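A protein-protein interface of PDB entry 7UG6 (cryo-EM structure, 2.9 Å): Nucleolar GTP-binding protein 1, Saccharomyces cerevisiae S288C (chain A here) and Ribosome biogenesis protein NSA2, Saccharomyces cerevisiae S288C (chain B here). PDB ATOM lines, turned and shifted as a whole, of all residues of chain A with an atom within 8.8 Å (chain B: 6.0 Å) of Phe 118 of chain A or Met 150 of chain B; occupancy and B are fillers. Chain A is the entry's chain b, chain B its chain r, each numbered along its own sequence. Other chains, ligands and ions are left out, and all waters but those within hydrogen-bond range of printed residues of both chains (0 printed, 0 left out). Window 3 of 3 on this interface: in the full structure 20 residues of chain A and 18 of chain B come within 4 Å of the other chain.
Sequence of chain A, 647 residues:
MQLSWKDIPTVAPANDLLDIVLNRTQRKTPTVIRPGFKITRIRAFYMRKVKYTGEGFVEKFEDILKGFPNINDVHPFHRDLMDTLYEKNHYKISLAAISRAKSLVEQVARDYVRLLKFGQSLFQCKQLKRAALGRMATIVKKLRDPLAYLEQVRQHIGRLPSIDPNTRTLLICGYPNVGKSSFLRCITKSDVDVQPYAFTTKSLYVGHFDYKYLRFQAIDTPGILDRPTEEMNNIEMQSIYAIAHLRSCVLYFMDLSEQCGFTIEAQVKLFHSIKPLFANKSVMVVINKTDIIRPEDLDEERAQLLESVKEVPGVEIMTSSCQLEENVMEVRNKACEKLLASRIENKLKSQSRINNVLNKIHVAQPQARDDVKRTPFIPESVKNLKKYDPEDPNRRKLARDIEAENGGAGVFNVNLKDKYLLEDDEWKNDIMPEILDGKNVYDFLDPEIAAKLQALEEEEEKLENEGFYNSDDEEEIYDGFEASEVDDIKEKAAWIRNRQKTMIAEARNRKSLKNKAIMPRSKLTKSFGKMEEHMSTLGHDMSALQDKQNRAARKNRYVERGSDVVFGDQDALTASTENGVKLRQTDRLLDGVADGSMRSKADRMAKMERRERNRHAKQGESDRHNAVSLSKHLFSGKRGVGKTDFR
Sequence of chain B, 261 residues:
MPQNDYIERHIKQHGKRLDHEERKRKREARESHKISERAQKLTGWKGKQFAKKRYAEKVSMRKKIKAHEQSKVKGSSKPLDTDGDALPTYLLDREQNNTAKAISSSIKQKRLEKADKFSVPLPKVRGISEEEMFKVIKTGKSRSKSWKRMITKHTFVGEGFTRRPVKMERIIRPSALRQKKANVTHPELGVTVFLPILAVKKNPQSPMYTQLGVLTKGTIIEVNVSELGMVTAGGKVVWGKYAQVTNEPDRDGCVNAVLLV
Of chain B, only Met 150 (3.3 Å), Pro 174 (3.7 Å), Ala 176 (3.5 Å) and Leu 177 (3.7 Å) come within 4 Å of Phe 118 of chain A.
Printed residues of chain A within 4 Å of Met 150 of chain B: Phe 118.
Of the printed residues of chain A, Lys 135 of chain B touches Gln 120 (3.7 Å).
Printed residues of chain A within 4 Å of Ala 176 of chain B: Phe 118.
Leu 116 of chain A touches none of the printed residues of chain B.
The nearest residue of chain A that does not touch Met 150 of chain B is Gln 120 of chain A (5.8 Å).
Printed residues of chain B that touch a printed residue of chain A: Lys 135, Met 150, Thr 152, Pro 174, Ala 176 and Leu 177.
Hydrophobic or aromatic side chains of chain B that line the printed part of chain A: Met 150, Pro 174, Ala 176 and Leu 177.
Of the 17 printed residues of chain A, 3 touch a printed residue of chain B.
Hydrophobic or aromatic side chains of chain A that line the printed part of chain B: Leu 115 and Phe 118.
Among the printed residues, no Asp or Glu carboxylate lies within 4 Å of a Lys or Arg side-chain nitrogen of the other chain.
The backbone carbonyl oxygen of Phe 118 of chain A is in hydrogen-bond range of the side-chain amide nitrogen of Gln 120 of chain A (2.9 Å).
N of Gln 120 of chain A is in hydrogen-bond range of OE1 of Gln 124 of chain A (2.7 Å).
The backbone carbonyl oxygen (O) of Met 133 of chain B lies within hydrogen-bond range of the backbone NH (N) of Thr 152 of chain B, 2.6 Å away.
The backbone NH of Lys 135 of chain B lies within hydrogen-bond range of the backbone carbonyl oxygen of Met 150 of chain B.
CD2 of Leu 115 of chain A touches CD1 of Leu 177 of chain B (3.95 Å).
Phe 118 of chain A touches Met 150 of chain B.
Pro 174 of chain B touches Phe 118 of chain A (CB to CE1, 3.7 Å).
Phe 118 of chain A touches Ala 176 of chain B.
CD1 of Leu 177 of chain B touches CD2 of Phe 118 of chain A (3.7 Å).
OE1 of Gln 120 of chain A touches CG of Lys 135 of chain B (3.7 Å).
Gln 120 of chain A touches Thr 152 of chain B (NE2 to CG2, 3.5 Å).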
ATOM      1  N   ILE A  39     -14.260   7.954 -32.520  1.00  0.00           N
ATOM      2  CA  ILE A  39     -14.189   7.328 -31.207  1.00  0.00           C
ATOM      3  C   ILE A  39     -15.392   6.434 -30.977  1.00  0.00           C
ATOM      4  O   ILE A  39     -15.326   5.490 -30.185  1.00  0.00           O
ATOM      5  CB  ILE A  39     -14.047   8.384 -30.102  1.00  0.00           C
ATOM      6  CG1 ILE A  39     -13.657   7.716 -28.788  1.00  0.00           C
ATOM      7  CG2 ILE A  39     -15.335   9.151 -29.940  1.00  0.00           C
ATOM      8  CD1 ILE A  39     -12.469   6.797 -28.889  1.00  0.00           C
ATOM      9  N   ARG A  43     -14.874   2.708 -29.591  1.00  0.00           N
ATOM     10  CA  ARG A  43     -15.633   2.259 -28.441  1.00  0.00           C
ATOM     11  C   ARG A  43     -16.427   1.017 -28.773  1.00  0.00           C
ATOM     12  O   ARG A  43     -16.385   0.044 -28.028  1.00  0.00           O
ATOM     13  CB  ARG A  43     -16.563   3.355 -27.955  1.00  0.00           C
ATOM     14  CG  ARG A  43     -15.902   4.481 -27.249  1.00  0.00           C
ATOM     15  CD  ARG A  43     -16.975   5.379 -26.757  1.00  0.00           C
ATOM     16  NE  ARG A  43     -16.540   6.751 -26.619  1.00  0.00           N
ATOM     17  CZ  ARG A  43     -17.370   7.774 -26.690  1.00  0.00           C
ATOM     18  NH1 ARG A  43     -18.654   7.547 -26.906  1.00  0.00           N
ATOM     19  NH2 ARG A  43     -16.923   9.011 -26.557  1.00  0.00           N
ATOM     20  N   MET A  47     -16.108  -2.421 -26.647  1.00  0.00           N
ATOM     21  CA  MET A  47     -17.294  -2.980 -26.010  1.00  0.00           C
ATOM     22  C   MET A  47     -17.665  -4.322 -26.606  1.00  0.00           C
ATOM     23  O   MET A  47     -18.116  -5.203 -25.876  1.00  0.00           O
ATOM     24  CB  MET A  47     -18.478  -2.016 -26.102  1.00  0.00           C
ATOM     25  CG  MET A  47     -18.132  -0.581 -25.825  1.00  0.00           C
ATOM     26  SD  MET A  47     -19.438   0.644 -25.927  1.00  0.00           S
ATOM     27  CE  MET A  47     -20.720  -0.055 -24.926  1.00  0.00           C
ATOM     28  N   ASP A 111     -19.407  -3.711 -15.922  1.00  0.00           N
ATOM     29  CA  ASP A 111     -18.654  -2.550 -15.459  1.00  0.00           C
ATOM     30  C   ASP A 111     -17.802  -1.969 -16.570  1.00  0.00           C
ATOM     31  O   ASP A 111     -17.777  -0.753 -16.778  1.00  0.00           O
ATOM     32  CB  ASP A 111     -17.769  -2.927 -14.278  1.00  0.00           C
ATOM     33  CG  ASP A 111     -18.560  -3.346 -13.079  1.00  0.00           C
ATOM     34  OD1 ASP A 111     -19.801  -3.262 -13.137  1.00  0.00           O
ATOM     35  OD2 ASP A 111     -17.943  -3.761 -12.078  1.00  0.00           O
ATOM     36  N   TYR A 112     -17.105  -2.822 -17.309  1.00  0.00           N
ATOM     37  CA  TYR A 112     -16.167  -2.292 -18.283  1.00  0.00           C
ATOM     38  C   TYR A 112     -16.819  -1.928 -19.601  1.00  0.00           C
ATOM     39  O   TYR A 112     -16.233  -1.170 -20.372  1.00  0.00           O
ATOM     40  CB  TYR A 112     -15.045  -3.282 -18.488  1.00  0.00           C
ATOM     41  CG  TYR A 112     -14.093  -3.236 -17.336  1.00  0.00           C
ATOM     42  CD1 TYR A 112     -14.349  -3.942 -16.183  1.00  0.00           C
ATOM     43  CD2 TYR A 112     -12.971  -2.448 -17.380  1.00  0.00           C
ATOM     44  CE1 TYR A 112     -13.501  -3.887 -15.126  1.00  0.00           C
ATOM     45  CE2 TYR A 112     -12.120  -2.391 -16.327  1.00  0.00           C
ATOM     46  CZ  TYR A 112     -12.387  -3.113 -15.203  1.00  0.00           C
ATOM     47  OH  TYR A 112     -11.531  -3.058 -14.137  1.00  0.00           O
ATOM     48  N   VAL A 113     -18.015  -2.432 -19.879  1.00  0.00           N
ATOM     49  CA  VAL A 113     -18.810  -1.851 -20.948  1.00  0.00           C
ATOM     50  C   VAL A 113     -19.267  -0.453 -20.571  1.00  0.00           C
ATOM     51  O   VAL A 113     -19.269   0.455 -21.408  1.00  0.00           O
ATOM     52  CB  VAL A 113     -19.980  -2.782 -21.288  1.00  0.00           C
ATOM     53  CG1 VAL A 113     -20.908  -2.130 -22.216  1.00  0.00           C
ATOM     54  CG2 VAL A 113     -19.443  -3.996 -21.981  1.00  0.00           C
ATOM     55  N   ARG A 114     -19.643  -0.240 -19.307  1.00  0.00           N
ATOM     56  CA  ARG A 114     -19.997   1.115 -18.897  1.00  0.00           C
ATOM     57  C   ARG A 114     -18.806   2.058 -18.935  1.00  0.00           C
ATOM     58  O   ARG A 114     -18.957   3.223 -19.299  1.00  0.00           O
ATOM     59  CB  ARG A 114     -20.623   1.131 -17.508  1.00  0.00           C
ATOM     60  CG  ARG A 114     -22.120   1.060 -17.550  1.00  0.00           C
ATOM     61  CD  ARG A 114     -22.722   1.286 -16.195  1.00  0.00           C
ATOM     62  NE  ARG A 114     -22.543   0.138 -15.321  1.00  0.00           N
ATOM     63  CZ  ARG A 114     -22.811   0.154 -14.022  1.00  0.00           C
ATOM     64  NH1 ARG A 114     -23.271   1.260 -13.453  1.00  0.00           N
ATOM     65  NH2 ARG A 114     -22.617  -0.934 -13.289  1.00  0.00           N
ATOM     66  N   LEU A 115     -17.630   1.596 -18.543  1.00  0.00           N
ATOM     67  CA  LEU A 115     -16.473   2.480 -18.570  1.00  0.00           C
ATOM     68  C   LEU A 115     -16.021   2.803 -19.985  1.00  0.00           C
ATOM     69  O   LEU A 115     -15.596   3.928 -20.256  1.00  0.00           O
ATOM     70  CB  LEU A 115     -15.323   1.856 -17.788  1.00  0.00           C
ATOM     71  CG  LEU A 115     -15.614   1.708 -16.306  1.00  0.00           C
ATOM     72  CD1 LEU A 115     -14.509   0.938 -15.679  1.00  0.00           C
ATOM     73  CD2 LEU A 115     -15.744   3.055 -15.663  1.00  0.00           C
ATOM     74  N   LEU A 116     -16.094   1.830 -20.890  1.00  0.00           N
ATOM     75  CA  LEU A 116     -15.745   2.057 -22.284  1.00  0.00           C
ATOM     76  C   LEU A 116     -16.687   3.037 -22.945  1.00  0.00           C
ATOM     77  O   LEU A 116     -16.300   3.705 -23.907  1.00  0.00           O
ATOM     78  CB  LEU A 116     -15.769   0.737 -23.038  1.00  0.00           C
ATOM     79  CG  LEU A 116     -14.508  -0.098 -22.905  1.00  0.00           C
ATOM     80  CD1 LEU A 116     -14.776  -1.520 -23.297  1.00  0.00           C
ATOM     81  CD2 LEU A 116     -13.452   0.489 -23.778  1.00  0.00           C
ATOM     82  N   LYS A 117     -17.910   3.134 -22.438  1.00  0.00           N
ATOM     83  CA  LYS A 117     -18.894   4.082 -22.938  1.00  0.00           C
ATOM     84  C   LYS A 117     -18.387   5.512 -22.865  1.00  0.00           C
ATOM     85  O   LYS A 117     -18.835   6.369 -23.628  1.00  0.00           O
ATOM     86  CB  LYS A 117     -20.163   3.908 -22.120  1.00  0.00           C
ATOM     87  CG  LYS A 117     -21.311   4.769 -22.477  1.00  0.00           C
ATOM     88  CD  LYS A 117     -22.462   4.538 -21.534  1.00  0.00           C
ATOM     89  CE  LYS A 117     -22.857   3.083 -21.495  1.00  0.00           C
ATOM     90  NZ  LYS A 117     -22.972   2.497 -22.854  1.00  0.00           N
ATOM     91  N   PHE A 118     -17.451   5.789 -21.957  1.00  0.00           N
ATOM     92  CA  PHE A 118     -16.887   7.117 -21.772  1.00  0.00           C
ATOM     93  C   PHE A 118     -15.429   7.189 -22.190  1.00  0.00           C
ATOM     94  O   PHE A 118     -14.748   8.158 -21.862  1.00  0.00           O
ATOM     95  CB  PHE A 118     -17.027   7.551 -20.318  1.00  0.00           C
ATOM     96  CG  PHE A 118     -18.421   7.480 -19.812  1.00  0.00           C
ATOM     97  CD1 PHE A 118     -19.291   8.510 -20.029  1.00  0.00           C
ATOM     98  CD2 PHE A 118     -18.867   6.375 -19.139  1.00  0.00           C
ATOM     99  CE1 PHE A 118     -20.571   8.450 -19.575  1.00  0.00           C
ATOM    100  CE2 PHE A 118     -20.148   6.308 -18.692  1.00  0.00           C
ATOM    101  CZ  PHE A 118     -21.001   7.352 -18.903  1.00  0.00           C
ATOM    102  N   GLY A 119     -14.932   6.172 -22.886  1.00  0.00           N
ATOM    103  CA  GLY A 119     -13.560   6.221 -23.349  1.00  0.00           C
ATOM    104  C   GLY A 119     -13.369   7.337 -24.357  1.00  0.00           C
ATOM    105  O   GLY A 119     -14.227   7.591 -25.202  1.00  0.00           O
ATOM    106  N   GLN A 120     -12.231   8.012 -24.259  1.00  0.00           N
ATOM    107  CA  GLN A 120     -11.963   9.181 -25.075  1.00  0.00           C
ATOM    108  C   GLN A 120     -10.913   8.949 -26.142  1.00  0.00           C
ATOM    109  O   GLN A 120     -10.753   9.800 -27.021  1.00  0.00           O
ATOM    110  CB  GLN A 120     -11.521  10.351 -24.194  1.00  0.00           C
ATOM    111  CG  GLN A 120     -12.488  10.692 -23.091  1.00  0.00           C
ATOM    112  CD  GLN A 120     -13.808  11.190 -23.614  1.00  0.00           C
ATOM    113  OE1 GLN A 120     -13.862  11.852 -24.645  1.00  0.00           O
ATOM    114  NE2 GLN A 120     -14.882  10.887 -22.901  1.00  0.00           N
ATOM    115  N   SER A 121     -10.197   7.835 -26.096  1.00  0.00           N
ATOM    116  CA  SER A 121      -9.101   7.601 -27.016  1.00  0.00           C
ATOM    117  C   SER A 121      -8.979   6.109 -27.242  1.00  0.00           C
ATOM    118  O   SER A 121      -9.505   5.307 -26.470  1.00  0.00           O
ATOM    119  CB  SER A 121      -7.791   8.173 -26.477  1.00  0.00           C
ATOM    120  OG  SER A 121      -6.707   7.835 -27.319  1.00  0.00           O
ATOM    121  N   GLN A 124      -6.957   4.656 -24.173  1.00  0.00           N
ATOM    122  CA  GLN A 124      -7.734   4.411 -22.967  1.00  0.00           C
ATOM    123  C   GLN A 124      -8.702   3.261 -23.165  1.00  0.00           C
ATOM    124  O   GLN A 124      -8.863   2.421 -22.278  1.00  0.00           O
ATOM    125  CB  GLN A 124      -8.486   5.671 -22.553  1.00  0.00           C
ATOM    126  CG  GLN A 124      -9.325   5.489 -21.301  1.00  0.00           C
ATOM    127  CD  GLN A 124     -10.481   6.457 -21.228  1.00  0.00           C
ATOM    128  OE1 GLN A 124     -10.695   7.244 -22.141  1.00  0.00           O
ATOM    129  NE2 GLN A 124     -11.241   6.398 -20.145  1.00  0.00           N
ATOM    130  N   CYS A 125      -9.355   3.201 -24.321  1.00  0.00           N
ATOM    131  CA  CYS A 125     -10.299   2.118 -24.559  1.00  0.00           C
ATOM    132  C   CYS A 125      -9.584   0.782 -24.660  1.00  0.00           C
ATOM    133  O   CYS A 125     -10.105  -0.244 -24.215  1.00  0.00           O
ATOM    134  CB  CYS A 125     -11.110   2.392 -25.814  1.00  0.00           C
ATOM    135  SG  CYS A 125     -12.192   3.817 -25.701  1.00  0.00           S
ATOM    136  N   LEU A 128      -8.884  -0.250 -21.177  1.00  0.00           N
ATOM    137  CA  LEU A 128     -10.085  -0.732 -20.509  1.00  0.00           C
ATOM    138  C   LEU A 128     -10.459  -2.132 -20.977  1.00  0.00           C
ATOM    139  O   LEU A 128     -10.841  -2.980 -20.164  1.00  0.00           O
ATOM    140  CB  LEU A 128     -11.232   0.237 -20.737  1.00  0.00           C
ATOM    141  CG  LEU A 128     -11.176   1.514 -19.918  1.00  0.00           C
ATOM    142  CD1 LEU A 128     -12.104   2.518 -20.521  1.00  0.00           C
ATOM    143  CD2 LEU A 128     -11.579   1.222 -18.510  1.00  0.00           C
ATOM    144  N   MET B 133      -9.167  16.720 -19.100  1.00  0.00           N
ATOM    145  CA  MET B 133     -10.125  16.456 -18.031  1.00  0.00           C
ATOM    146  C   MET B 133     -11.557  16.540 -18.531  1.00  0.00           C
ATOM    147  O   MET B 133     -12.370  15.653 -18.261  1.00  0.00           O
ATOM    148  CB  MET B 133      -9.933  17.448 -16.888  1.00  0.00           C
ATOM    149  CG  MET B 133      -8.649  17.366 -16.114  1.00  0.00           C
ATOM    150  SD  MET B 133      -8.456  15.789 -15.300  1.00  0.00           S
ATOM    151  CE  MET B 133      -9.737  15.945 -14.083  1.00  0.00           C
ATOM    152  N   PHE B 134     -11.887  17.603 -19.249  1.00  0.00           N
ATOM    153  CA  PHE B 134     -13.267  17.967 -19.519  1.00  0.00           C
ATOM    154  C   PHE B 134     -13.615  17.690 -20.969  1.00  0.00           C
ATOM    155  O   PHE B 134     -12.851  18.027 -21.873  1.00  0.00           O
ATOM    156  CB  PHE B 134     -13.507  19.437 -19.206  1.00  0.00           C
ATOM    157  CG  PHE B 134     -13.352  19.779 -17.764  1.00  0.00           C
ATOM    158  CD1 PHE B 134     -14.337  19.462 -16.859  1.00  0.00           C
ATOM    159  CD2 PHE B 134     -12.228  20.437 -17.316  1.00  0.00           C
ATOM    160  CE1 PHE B 134     -14.199  19.784 -15.540  1.00  0.00           C
ATOM    161  CE2 PHE B 134     -12.089  20.758 -15.995  1.00  0.00           C
ATOM    162  CZ  PHE B 134     -13.073  20.426 -15.106  1.00  0.00           C
ATOM    163  N   LYS B 135     -14.769  17.081 -21.181  1.00  0.00           N
ATOM    164  CA  LYS B 135     -15.299  16.840 -22.509  1.00  0.00           C
ATOM    165  C   LYS B 135     -16.440  17.813 -22.748  1.00  0.00           C
ATOM    166  O   LYS B 135     -17.373  17.886 -21.947  1.00  0.00           O
ATOM    167  CB  LYS B 135     -15.779  15.399 -22.633  1.00  0.00           C
ATOM    168  CG  LYS B 135     -15.870  14.876 -24.036  1.00  0.00           C
ATOM    169  CD  LYS B 135     -17.291  14.834 -24.503  1.00  0.00           C
ATOM    170  CE  LYS B 135     -17.401  14.073 -25.794  1.00  0.00           C
ATOM    171  NZ  LYS B 135     -18.783  14.075 -26.295  1.00  0.00           N
ATOM    172  N   VAL B 136     -16.356  18.569 -23.836  1.00  0.00           N
ATOM    173  CA  VAL B 136     -17.369  19.573 -24.122  1.00  0.00           C
ATOM    174  C   VAL B 136     -18.658  18.890 -24.545  1.00  0.00           C
ATOM    175  O   VAL B 136     -18.657  17.986 -25.389  1.00  0.00           O
ATOM    176  CB  VAL B 136     -16.873  20.541 -25.201  1.00  0.00           C
ATOM    177  CG1 VAL B 136     -17.923  21.579 -25.498  1.00  0.00           C
ATOM    178  CG2 VAL B 136     -15.603  21.197 -24.751  1.00  0.00           C
ATOM    179  N   ILE B 137     -19.767  19.318 -23.962  1.00  0.00           N
ATOM    180  CA  ILE B 137     -21.084  18.830 -24.326  1.00  0.00           C
ATOM    181  C   ILE B 137     -21.837  19.963 -24.993  1.00  0.00           C
ATOM    182  O   ILE B 137     -21.956  21.056 -24.431  1.00  0.00           O
ATOM    183  CB  ILE B 137     -21.849  18.294 -23.111  1.00  0.00           C
ATOM    184  CG1 ILE B 137     -21.138  17.083 -22.534  1.00  0.00           C
ATOM    185  CG2 ILE B 137     -23.261  17.940 -23.476  1.00  0.00           C
ATOM    186  CD1 ILE B 137     -21.701  16.668 -21.247  1.00  0.00           C
ATOM    187  N   LYS B 148     -21.696  23.340 -21.075  1.00  0.00           N
ATOM    188  CA  LYS B 148     -21.647  22.174 -20.209  1.00  0.00           C
ATOM    189  C   LYS B 148     -20.336  21.426 -20.394  1.00  0.00           C
ATOM    190  O   LYS B 148     -19.827  21.282 -21.505  1.00  0.00           O
ATOM    191  CB  LYS B 148     -22.817  21.250 -20.513  1.00  0.00           C
ATOM    192  CG  LYS B 148     -24.118  21.622 -19.842  1.00  0.00           C
ATOM    193  CD  LYS B 148     -25.258  20.903 -20.503  1.00  0.00           C
ATOM    194  CE  LYS B 148     -26.363  20.597 -19.545  1.00  0.00           C
ATOM    195  NZ  LYS B 148     -26.489  21.643 -18.525  1.00  0.00           N
ATOM    196  N   ARG B 149     -19.783  20.950 -19.285  1.00  0.00           N
ATOM    197  CA  ARG B 149     -18.485  20.293 -19.293  1.00  0.00           C
ATOM    198  C   ARG B 149     -18.611  18.948 -18.612  1.00  0.00           C
ATOM    199  O   ARG B 149     -19.307  18.826 -17.604  1.00  0.00           O
ATOM    200  CB  ARG B 149     -17.436  21.134 -18.581  1.00  0.00           C
ATOM    201  CG  ARG B 149     -17.089  22.377 -19.317  1.00  0.00           C
ATOM    202  CD  ARG B 149     -16.327  22.044 -20.553  1.00  0.00           C
ATOM    203  NE  ARG B 149     -15.793  23.235 -21.188  1.00  0.00           N
ATOM    204  CZ  ARG B 149     -16.458  23.960 -22.070  1.00  0.00           C
ATOM    205  NH1 ARG B 149     -17.682  23.607 -22.430  1.00  0.00           N
ATOM    206  NH2 ARG B 149     -15.895  25.028 -22.599  1.00  0.00           N
ATOM    207  N   MET B 150     -17.946  17.944 -19.156  1.00  0.00           N
ATOM    208  CA  MET B 150     -18.059  16.586 -18.662  1.00  0.00           C
ATOM    209  C   MET B 150     -16.689  16.071 -18.277  1.00  0.00           C
ATOM    210  O   MET B 150     -15.783  16.047 -19.109  1.00  0.00           O
ATOM    211  CB  MET B 150     -18.659  15.687 -19.723  1.00  0.00           C
ATOM    212  CG  MET B 150     -18.873  14.311 -19.259  1.00  0.00           C
ATOM    213  SD  MET B 150     -19.661  13.378 -20.545  1.00  0.00           S
ATOM    214  CE  MET B 150     -19.674  11.816 -19.728  1.00  0.00           C
ATOM    215  N   ILE B 151     -16.543  15.644 -17.034  1.00  0.00           N
ATOM    216  CA  ILE B 151     -15.251  15.180 -16.558  1.00  0.00           C
ATOM    217  C   ILE B 151     -15.000  13.783 -17.092  1.00  0.00           C
ATOM    218  O   ILE B 151     -15.808  12.873 -16.892  1.00  0.00           O
ATOM    219  CB  ILE B 151     -15.193  15.213 -15.031  1.00  0.00           C
ATOM    220  CG1 ILE B 151     -15.431  16.630 -14.537  1.00  0.00           C
ATOM    221  CG2 ILE B 151     -13.869  14.702 -14.557  1.00  0.00           C
ATOM    222  CD1 ILE B 151     -15.173  16.798 -13.084  1.00  0.00           C
ATOM    223  N   THR B 152     -13.876  13.613 -17.781  1.00  0.00           N
ATOM    224  CA  THR B 152     -13.526  12.338 -18.376  1.00  0.00           C
ATOM    225  C   THR B 152     -12.786  11.419 -17.425  1.00  0.00           C
ATOM    226  O   THR B 152     -12.552  10.257 -17.769  1.00  0.00           O
ATOM    227  CB  THR B 152     -12.670  12.560 -19.616  1.00  0.00           C
ATOM    228  OG1 THR B 152     -11.565  13.397 -19.278  1.00  0.00           O
ATOM    229  CG2 THR B 152     -13.475  13.239 -20.683  1.00  0.00           C
ATOM    230  N   ARG B 170     -23.213  22.558 -14.987  1.00  0.00           N
ATOM    231  CA  ARG B 170     -22.132  22.768 -15.938  1.00  0.00           C
ATOM    232  C   ARG B 170     -21.168  21.601 -15.945  1.00  0.00           C
ATOM    233  O   ARG B 170     -20.855  21.051 -17.003  1.00  0.00           O
ATOM    234  CB  ARG B 170     -21.374  24.045 -15.614  1.00  0.00           C
ATOM    235  CG  ARG B 170     -20.353  24.398 -16.632  1.00  0.00           C
ATOM    236  CD  ARG B 170     -19.807  25.783 -16.441  1.00  0.00           C
ATOM    237  NE  ARG B 170     -19.065  25.945 -15.202  1.00  0.00           N
ATOM    238  CZ  ARG B 170     -19.249  26.941 -14.346  1.00  0.00           C
ATOM    239  NH1 ARG B 170     -20.138  27.883 -14.603  1.00  0.00           N
ATOM    240  NH2 ARG B 170     -18.523  27.008 -13.245  1.00  0.00           N
ATOM    241  N   ILE B 171     -20.674  21.224 -14.777  1.00  0.00           N
ATOM    242  CA  ILE B 171     -19.689  20.163 -14.662  1.00  0.00           C
ATOM    243  C   ILE B 171     -20.428  18.844 -14.547  1.00  0.00           C
ATOM    244  O   ILE B 171     -21.074  18.572 -13.532  1.00  0.00           O
ATOM    245  CB  ILE B 171     -18.775  20.389 -13.456  1.00  0.00           C
ATOM    246  CG1 ILE B 171     -18.048  21.715 -13.607  1.00  0.00           C
ATOM    247  CG2 ILE B 171     -17.798  19.265 -13.358  1.00  0.00           C
ATOM    248  CD1 ILE B 171     -17.146  21.761 -14.793  1.00  0.00           C
ATOM    249  N   ILE B 172     -20.347  18.031 -15.584  1.00  0.00           N
ATOM    250  CA  ILE B 172     -21.034  16.755 -15.622  1.00  0.00           C
ATOM    251  C   ILE B 172     -20.116  15.730 -14.991  1.00  0.00           C
ATOM    252  O   ILE B 172     -18.950  15.609 -15.378  1.00  0.00           O
ATOM    253  CB  ILE B 172     -21.385  16.350 -17.060  1.00  0.00           C
ATOM    254  CG1 ILE B 172     -22.232  17.416 -17.741  1.00  0.00           C
ATOM    255  CG2 ILE B 172     -22.131  15.043 -17.052  1.00  0.00           C
ATOM    256  CD1 ILE B 172     -23.514  17.665 -17.101  1.00  0.00           C
ATOM    257  N   ARG B 173     -20.626  15.001 -14.010  1.00  0.00           N
ATOM    258  CA  ARG B 173     -19.906  13.874 -13.425  1.00  0.00           C
ATOM    259  C   ARG B 173     -20.762  12.641 -13.616  1.00  0.00           C
ATOM    260  O   ARG B 173     -21.667  12.385 -12.804  1.00  0.00           O
ATOM    261  CB  ARG B 173     -19.622  14.109 -11.951  1.00  0.00           C
ATOM    262  CG  ARG B 173     -18.423  14.948 -11.703  1.00  0.00           C
ATOM    263  CD  ARG B 173     -18.389  15.349 -10.269  1.00  0.00           C
ATOM    264  NE  ARG B 173     -19.356  16.390  -9.988  1.00  0.00           N
ATOM    265  CZ  ARG B 173     -19.352  17.102  -8.872  1.00  0.00           C
ATOM    266  NH1 ARG B 173     -18.438  16.866  -7.948  1.00  0.00           N
ATOM    267  NH2 ARG B 173     -20.258  18.042  -8.686  1.00  0.00           N
ATOM    268  N   PRO B 174     -20.540  11.867 -14.674  1.00  0.00           N
ATOM    269  CA  PRO B 174     -21.432  10.747 -14.969  1.00  0.00           C
ATOM    270  C   PRO B 174     -21.412   9.711 -13.865  1.00  0.00           C
ATOM    271  O   PRO B 174     -20.385   9.473 -13.232  1.00  0.00           O
ATOM    272  CB  PRO B 174     -20.877  10.190 -16.277  1.00  0.00           C
ATOM    273  CG  PRO B 174     -19.503  10.653 -16.321  1.00  0.00           C
ATOM    274  CD  PRO B 174     -19.480  11.986 -15.676  1.00  0.00           C
ATOM    275  N   SER B 175     -22.570   9.096 -13.639  1.00  0.00           N
ATOM    276  CA  SER B 175     -22.724   8.195 -12.508  1.00  0.00           C
ATOM    277  C   SER B 175     -21.835   6.971 -12.634  1.00  0.00           C
ATOM    278  O   SER B 175     -21.536   6.319 -11.631  1.00  0.00           O
ATOM    279  CB  SER B 175     -24.185   7.778 -12.378  1.00  0.00           C
ATOM    280  OG  SER B 175     -24.387   6.992 -11.221  1.00  0.00           O
ATOM    281  N   ALA B 176     -21.405   6.638 -13.850  1.00  0.00           N
ATOM    282  CA  ALA B 176     -20.566   5.463 -14.030  1.00  0.00           C
ATOM    283  C   ALA B 176     -19.155   5.705 -13.544  1.00  0.00           C
ATOM    284  O   ALA B 176     -18.505   4.780 -13.050  1.00  0.00           O
ATOM    285  CB  ALA B 176     -20.540   5.041 -15.491  1.00  0.00           C
ATOM    286  N   LEU B 177     -18.666   6.927 -13.662  1.00  0.00           N
ATOM    287  CA  LEU B 177     -17.302   7.235 -13.274  1.00  0.00           C
ATOM    288  C   LEU B 177     -17.181   7.621 -11.810  1.00  0.00           C
ATOM    289  O   LEU B 177     -16.087   7.985 -11.374  1.00  0.00           O
ATOM    290  CB  LEU B 177     -16.746   8.350 -14.160  1.00  0.00           C
ATOM    291  CG  LEU B 177     -15.913   7.905 -15.362  1.00  0.00           C
ATOM    292  CD1 LEU B 177     -16.638   6.871 -16.181  1.00  0.00           C
ATOM    293  CD2 LEU B 177     -15.553   9.091 -16.224  1.00  0.00           C
